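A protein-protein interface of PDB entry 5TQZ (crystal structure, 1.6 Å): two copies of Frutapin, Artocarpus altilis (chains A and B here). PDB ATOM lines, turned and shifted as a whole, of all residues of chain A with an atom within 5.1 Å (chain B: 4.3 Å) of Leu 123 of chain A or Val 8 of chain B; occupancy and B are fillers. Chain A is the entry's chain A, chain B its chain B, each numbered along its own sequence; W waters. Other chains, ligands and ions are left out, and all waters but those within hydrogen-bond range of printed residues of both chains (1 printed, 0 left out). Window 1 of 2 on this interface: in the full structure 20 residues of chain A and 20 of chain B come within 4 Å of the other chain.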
ATOM      1  N   VAL A   8       6.505  32.985  33.796  1.00  0.00           N
ATOM      2  CA  VAL A   8       7.768  32.268  33.420  1.00  0.00           C
ATOM      3  C   VAL A   8       8.681  33.135  32.614  1.00  0.00           C
ATOM      4  O   VAL A   8       8.152  34.114  31.972  1.00  0.00           O
ATOM      5  CB  VAL A   8       7.460  30.927  32.731  1.00  0.00           C
ATOM      6  CG1 VAL A   8       6.721  30.043  33.603  1.00  0.00           C
ATOM      7  CG2 VAL A   8       6.728  31.124  31.486  1.00  0.00           C
ATOM      8  N   TRP A  11      13.285  35.551  29.237  1.00  0.00           N
ATOM      9  CA  TRP A  11      14.306  35.195  28.308  1.00  0.00           C
ATOM     10  C   TRP A  11      14.845  36.478  27.618  1.00  0.00           C
ATOM     11  O   TRP A  11      14.068  37.301  27.163  1.00  0.00           O
ATOM     12  CB  TRP A  11      13.906  34.128  27.313  1.00  0.00           C
ATOM     13  CG  TRP A  11      13.366  32.813  27.977  1.00  0.00           C
ATOM     14  CD1 TRP A  11      14.073  31.714  28.291  1.00  0.00           C
ATOM     15  CD2 TRP A  11      12.000  32.483  28.205  1.00  0.00           C
ATOM     16  NE1 TRP A  11      13.280  30.767  28.804  1.00  0.00           N
ATOM     17  CE2 TRP A  11      11.972  31.203  28.755  1.00  0.00           C
ATOM     18  CE3 TRP A  11      10.811  33.158  28.070  1.00  0.00           C
ATOM     19  CZ2 TRP A  11      10.776  30.538  29.119  1.00  0.00           C
ATOM     20  CZ3 TRP A  11       9.611  32.505  28.384  1.00  0.00           C
ATOM     21  CH2 TRP A  11       9.601  31.250  28.920  1.00  0.00           C
ATOM     22  N   VAL A  78      -0.157  27.683  21.988  1.00  0.00           N
ATOM     23  CA  VAL A  78       0.303  26.516  22.674  1.00  0.00           C
ATOM     24  C   VAL A  78       1.813  26.425  22.689  1.00  0.00           C
ATOM     25  O   VAL A  78       2.342  25.522  23.316  1.00  0.00           O
ATOM     26  CB  VAL A  78      -0.248  25.218  22.054  1.00  0.00           C
ATOM     27  CG1 VAL A  78      -1.755  25.153  22.073  1.00  0.00           C
ATOM     28  CG2 VAL A  78       0.276  25.122  20.570  1.00  0.00           C
ATOM     29  N   SER A  79       2.520  27.283  22.009  1.00  0.00           N
ATOM     30  CA  SER A  79       3.955  27.472  22.053  1.00  0.00           C
ATOM     31  C   SER A  79       4.385  28.898  21.789  1.00  0.00           C
ATOM     32  O   SER A  79       3.901  29.670  20.896  1.00  0.00           O
ATOM     33  CB  SER A  79       4.626  26.679  20.870  1.00  0.00           C
ATOM     34  OG  SER A  79       6.055  26.437  21.189  1.00  0.00           O
ATOM     35  N   VAL A  80       5.374  29.281  22.622  1.00  0.00           N
ATOM     36  CA  VAL A  80       6.207  30.469  22.429  1.00  0.00           C
ATOM     37  C   VAL A  80       7.642  29.997  22.396  1.00  0.00           C
ATOM     38  O   VAL A  80       8.096  29.321  23.298  1.00  0.00           O
ATOM     39  CB  VAL A  80       5.981  31.523  23.601  1.00  0.00           C
ATOM     40  CG1 VAL A  80       6.837  32.702  23.407  1.00  0.00           C
ATOM     41  CG2 VAL A  80       4.487  31.989  23.758  1.00  0.00           C
ATOM     42  N   SER A  81       8.420  30.396  21.387  1.00  0.00           N
ATOM     43  CA  SER A  81       9.825  30.102  21.324  1.00  0.00           C
ATOM     44  C   SER A  81      10.639  31.178  20.544  1.00  0.00           C
ATOM     45  O   SER A  81      10.110  32.200  20.004  1.00  0.00           O
ATOM     46  CB  SER A  81       9.999  28.771  20.788  1.00  0.00           C
ATOM     47  OG  SER A  81       9.719  28.676  19.314  1.00  0.00           O
ATOM     48  N   PHE A 121      15.101  29.282  23.233  1.00  0.00           N
ATOM     49  CA  PHE A 121      14.164  29.186  24.358  1.00  0.00           C
ATOM     50  C   PHE A 121      12.910  28.616  23.766  1.00  0.00           C
ATOM     51  O   PHE A 121      12.545  28.844  22.605  1.00  0.00           O
ATOM     52  CB  PHE A 121      13.938  30.401  25.257  1.00  0.00           C
ATOM     53  CG  PHE A 121      13.239  31.557  24.557  1.00  0.00           C
ATOM     54  CD1 PHE A 121      13.921  32.372  23.757  1.00  0.00           C
ATOM     55  CD2 PHE A 121      11.865  31.685  24.640  1.00  0.00           C
ATOM     56  CE1 PHE A 121      13.316  33.527  23.166  1.00  0.00           C
ATOM     57  CE2 PHE A 121      11.226  32.747  24.038  1.00  0.00           C
ATOM     58  CZ  PHE A 121      11.929  33.636  23.237  1.00  0.00           C
ATOM     59  N   ASN A 122      12.250  27.823  24.589  1.00  0.00           N
ATOM     60  CA  ASN A 122      11.052  27.094  24.071  1.00  0.00           C
ATOM     61  C   ASN A 122      10.119  26.813  25.187  1.00  0.00           C
ATOM     62  O   ASN A 122      10.476  25.951  26.094  1.00  0.00           O
ATOM     63  CB  ASN A 122      11.579  25.847  23.393  1.00  0.00           C
ATOM     64  CG  ASN A 122      10.510  24.754  23.076  1.00  0.00           C
ATOM     65  OD1 ASN A 122       9.359  25.091  22.757  1.00  0.00           O
ATOM     66  ND2 ASN A 122      10.914  23.530  23.096  1.00  0.00           N
ATOM     67  N   LEU A 123       8.888  27.380  25.085  1.00  0.00           N
ATOM     68  CA  LEU A 123       7.814  27.147  26.058  1.00  0.00           C
ATOM     69  C   LEU A 123       6.573  26.437  25.406  1.00  0.00           C
ATOM     70  O   LEU A 123       5.660  27.095  24.939  1.00  0.00           O
ATOM     71  CB  LEU A 123       7.386  28.420  26.663  1.00  0.00           C
ATOM     72  CG  LEU A 123       6.360  28.378  27.836  1.00  0.00           C
ATOM     73  CD1 LEU A 123       6.906  27.838  29.144  1.00  0.00           C
ATOM     74  CD2 LEU A 123       5.646  29.658  28.058  1.00  0.00           C
ATOM     75  N   PRO A 124       6.609  25.128  25.309  1.00  0.00           N
ATOM     76  CA  PRO A 124       5.385  24.400  24.910  1.00  0.00           C
ATOM     77  C   PRO A 124       4.398  24.468  26.081  1.00  0.00           C
ATOM     78  O   PRO A 124       4.840  24.184  27.242  1.00  0.00           O
ATOM     79  CB  PRO A 124       5.850  22.991  24.759  1.00  0.00           C
ATOM     80  CG  PRO A 124       7.327  22.946  24.951  1.00  0.00           C
ATOM     81  CD  PRO A 124       7.614  24.166  25.752  1.00  0.00           C
ATOM     82  N   ILE A 125       3.062  24.628  25.820  1.00  0.00           N
ATOM     83  CA  ILE A 125       2.033  24.841  26.860  1.00  0.00           C
ATOM     84  C   ILE A 125       1.174  23.682  26.697  1.00  0.00           C
ATOM     85  O   ILE A 125       0.551  23.528  25.611  1.00  0.00           O
ATOM     86  CB  ILE A 125       1.299  26.193  26.744  1.00  0.00           C
ATOM     87  CG1 ILE A 125       2.170  27.444  26.952  1.00  0.00           C
ATOM     88  CG2 ILE A 125       0.243  26.303  27.769  1.00  0.00           C
ATOM     89  CD1 ILE A 125       1.672  28.785  26.432  1.00  0.00           C
ATOM     90  N   GLU A 126       1.194  22.722  27.635  1.00  0.00           N
ATOM     91  CA  GLU A 126       0.376  21.533  27.544  1.00  0.00           C
ATOM     92  C   GLU A 126      -1.055  21.844  28.065  1.00  0.00           C
ATOM     93  O   GLU A 126      -2.109  21.457  27.549  1.00  0.00           O
ATOM     94  CB  GLU A 126       0.951  20.352  28.319  1.00  0.00           C
ATOM     95  CG  GLU A 126       0.025  19.201  28.481  1.00  0.00           C
ATOM     96  CD  GLU A 126       0.779  17.893  28.704  1.00  0.00           C
ATOM     97  OE1 GLU A 126       2.068  17.905  28.835  1.00  0.00           O
ATOM     98  OE2 GLU A 126       0.267  16.812  28.364  1.00  0.00           O
ATOM     99  N   VAL A 146       6.250  35.538  30.045  1.00  0.00           N
ATOM    100  CA  VAL A 146       4.817  35.303  29.881  1.00  0.00           C
ATOM    101  C   VAL A 146       4.080  34.933  31.137  1.00  0.00           C
ATOM    102  O   VAL A 146       4.563  34.146  32.020  1.00  0.00           O
ATOM    103  CB  VAL A 146       4.353  34.220  28.900  1.00  0.00           C
ATOM    104  CG1 VAL A 146       4.220  34.899  27.560  1.00  0.00           C
ATOM    105  CG2 VAL A 146       5.178  32.981  29.011  1.00  0.00           C
ATOM    106  N   MET A 148       0.594  33.392  32.759  1.00  0.00           N
ATOM    107  CA  MET A 148      -0.211  32.167  32.376  1.00  0.00           C
ATOM    108  C   MET A 148      -1.338  31.959  33.458  1.00  0.00           C
ATOM    109  O   MET A 148      -1.118  32.247  34.635  1.00  0.00           O
ATOM    110  CB  MET A 148       0.670  30.895  32.299  1.00  0.00           C
ATOM    111  CG  MET A 148       1.844  31.028  31.381  1.00  0.00           C
ATOM    112  SD  MET A 148       2.770  29.443  31.362  1.00  0.00           S
ATOM    113  CE  MET A 148       1.497  28.509  30.565  1.00  0.00           C
ATOM    114  N   THR B   7       0.456  23.202  33.011  1.00  0.00           N
ATOM    115  CA  THR B   7       1.465  22.230  32.728  1.00  0.00           C
ATOM    116  C   THR B   7       2.194  22.674  31.464  1.00  0.00           C
ATOM    117  O   THR B   7       1.642  23.180  30.488  1.00  0.00           O
ATOM    118  CB  THR B   7       0.825  20.871  32.430  1.00  0.00           C
ATOM    119  OG1 THR B   7      -0.018  20.563  33.508  1.00  0.00           O
ATOM    120  CG2 THR B   7       1.792  19.816  32.235  1.00  0.00           C
ATOM    121  N   VAL B   8       3.507  22.569  31.551  1.00  0.00           N
ATOM    122  CA  VAL B   8       4.402  22.983  30.416  1.00  0.00           C
ATOM    123  C   VAL B   8       5.363  21.814  30.069  1.00  0.00           C
ATOM    124  O   VAL B   8       5.617  20.923  30.866  1.00  0.00           O
ATOM    125  CB  VAL B   8       5.268  24.279  30.657  1.00  0.00           C
ATOM    126  CG1 VAL B   8       4.441  25.572  30.726  1.00  0.00           C
ATOM    127  CG2 VAL B   8       6.061  24.144  31.960  1.00  0.00           C
ATOM    128  N   GLY B   9       5.864  21.863  28.852  1.00  0.00           N
ATOM    129  CA  GLY B   9       6.475  20.793  28.284  1.00  0.00           C
ATOM    130  C   GLY B   9       5.560  20.052  27.373  1.00  0.00           C
ATOM    131  O   GLY B   9       4.484  20.570  27.030  1.00  0.00           O
ATOM    132  N   TRP B  11       9.473  18.555  27.121  1.00  0.00           N
ATOM    133  CA  TRP B  11      10.835  18.558  26.482  1.00  0.00           C
ATOM    134  C   TRP B  11      11.455  17.176  26.346  1.00  0.00           C
ATOM    135  O   TRP B  11      11.509  16.384  27.391  1.00  0.00           O
ATOM    136  CB  TRP B  11      11.693  19.479  27.250  1.00  0.00           C
ATOM    137  CG  TRP B  11      11.262  20.912  27.323  1.00  0.00           C
ATOM    138  CD1 TRP B  11      11.378  21.803  26.335  1.00  0.00           C
ATOM    139  CD2 TRP B  11      10.601  21.519  28.448  1.00  0.00           C
ATOM    140  NE1 TRP B  11      10.887  23.107  26.854  1.00  0.00           N
ATOM    141  CE2 TRP B  11      10.414  22.929  28.128  1.00  0.00           C
ATOM    142  CE3 TRP B  11      10.174  21.076  29.716  1.00  0.00           C
ATOM    143  CZ2 TRP B  11       9.734  23.781  28.973  1.00  0.00           C
ATOM    144  CZ3 TRP B  11       9.611  21.990  30.598  1.00  0.00           C
ATOM    145  CH2 TRP B  11       9.500  23.358  30.232  1.00  0.00           C
ATOM    146  N   LEU B 123      13.304  26.525  31.659  1.00  0.00           N
ATOM    147  CA  LEU B 123      12.114  27.119  32.305  1.00  0.00           C
ATOM    148  C   LEU B 123      12.550  27.947  33.578  1.00  0.00           C
ATOM    149  O   LEU B 123      12.434  27.395  34.732  1.00  0.00           O
ATOM    150  CB  LEU B 123      11.212  26.038  32.640  1.00  0.00           C
ATOM    151  CG  LEU B 123       9.807  26.379  33.232  1.00  0.00           C
ATOM    152  CD1 LEU B 123       8.976  27.049  32.163  1.00  0.00           C
ATOM    153  CD2 LEU B 123       9.056  25.263  33.916  1.00  0.00           C
ATOM    154  N   GLY B 145       8.312  17.098  31.786  1.00  0.00           N
ATOM    155  CA  GLY B 145       7.378  18.292  31.789  1.00  0.00           C
ATOM    156  C   GLY B 145       7.054  18.554  33.253  1.00  0.00           C
ATOM    157  O   GLY B 145       7.350  17.768  34.126  1.00  0.00           O
ATOM    158  N   VAL B 146       6.400  19.669  33.483  1.00  0.00           N
ATOM    159  CA  VAL B 146       6.244  20.236  34.868  1.00  0.00           C
ATOM    160  C   VAL B 146       4.841  20.816  35.006  1.00  0.00           C
ATOM    161  O   VAL B 146       4.355  21.505  34.167  1.00  0.00           O
ATOM    162  CB  VAL B 146       7.162  21.374  35.365  1.00  0.00           C
ATOM    163  CG1 VAL B 146       8.568  20.804  35.481  1.00  0.00           C
ATOM    164  CG2 VAL B 146       7.133  22.445  34.428  1.00  0.00           C
HETATM  165  O   HOH W   1       4.626  18.361  30.036  1.00  0.00           O
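Val 78 of chain A touches none of the printed residues of chain B. Of the printed residues of chain B, Asn 122 of chain A touches Trp 11 (3.0 Å). Printed residues of chain B within 4 Å of Leu 123 of chain A: Val 8 (3.7 Å) and Leu 123 (3.7 Å). Printed residues of chain B within 4 Å of Pro 124 of chain A: Val 8, Gly 9 and Trp 11. Of the printed residues of chain B, Ile 125 of chain A touches Thr 7 (3.9 Å). Printed residues of chain A within 4 Å of Thr 7 of chain B: Ile 125 (3.9 Å) and Glu 126 (2.9 Å). Of the printed residues of chain A, Gly 9 of chain B touches Pro 124 (3.0 Å) and Glu 126 (3.8 Å). Val 146 of chain B touches none of the printed residues of chain A. The nearest printed residue of chain A that does not touch Thr 7 of chain B is Pro 124 of chain A (4.7 Å).
O of Val 146 of chain B lies within hydrogen-bond range of N of Val 8 of chain B, at 2.9 Å. The backbone carbonyl oxygen (O) of Val 78 of chain A is in hydrogen-bond range of the backbone NH (N) of Ile 125 of chain A, 2.8 Å away. O of Val 80 of chain A lies within hydrogen-bond range of N of Leu 123 of chain A, at 2.8 Å.
Leu 123 of chain A touches Val 8 of chain B. Leu 123 of chain A touches Leu 123 of chain B. O of Pro 124 of chain A touches CA of Val 8 of chain B (3.4 Å). CD of Pro 124 of chain A touches NE1 of Trp 11 of chain B (3.6 Å). Ile 125 of chain A touches Thr 7 of chain B. Glu 126 of chain A touches Gly 9 of chain B (CB to O, 3.8 Å).
Water W1 lies within hydrogen-bond range of OE1 of Glu 126 of chain A (2.9 Å) and O of Val 8 of chain B (2.9 Å).
The backbone carbonyl oxygen (O) of Pro 124 of chain A sits at hydrogen-bond distance from the backbone NH (N) of Gly 9 of chain B, 3.0 Å away. O of Asn 122 of chain A is in hydrogen-bond range of NE1 of Trp 11 of chain B (3.0 Å). N of Glu 126 of chain A sits at hydrogen-bond distance from O of Thr 7 of chain B, 2.9 Å away.
Of the 7 printed residues of chain B, 5 touch a printed residue of chain A. Along chain B the printed residues that touch a printed residue of chain A span positions 7 to 123. Along chain A the printed residues that touch a printed residue of chain B span positions 122 to 126.
Leu 123 of chain A touches Val 8 of chain B, but with the chains exchanged Val 8 of chain A does not touch Leu 123 of chain B (4.02 Å). Leu 123 of chain A touches its own counterpart, Leu 123 of chain B. Of the 9 pairs that touch across the chains among the printed residues, 1 has its exchanged pair printed and touching as well.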
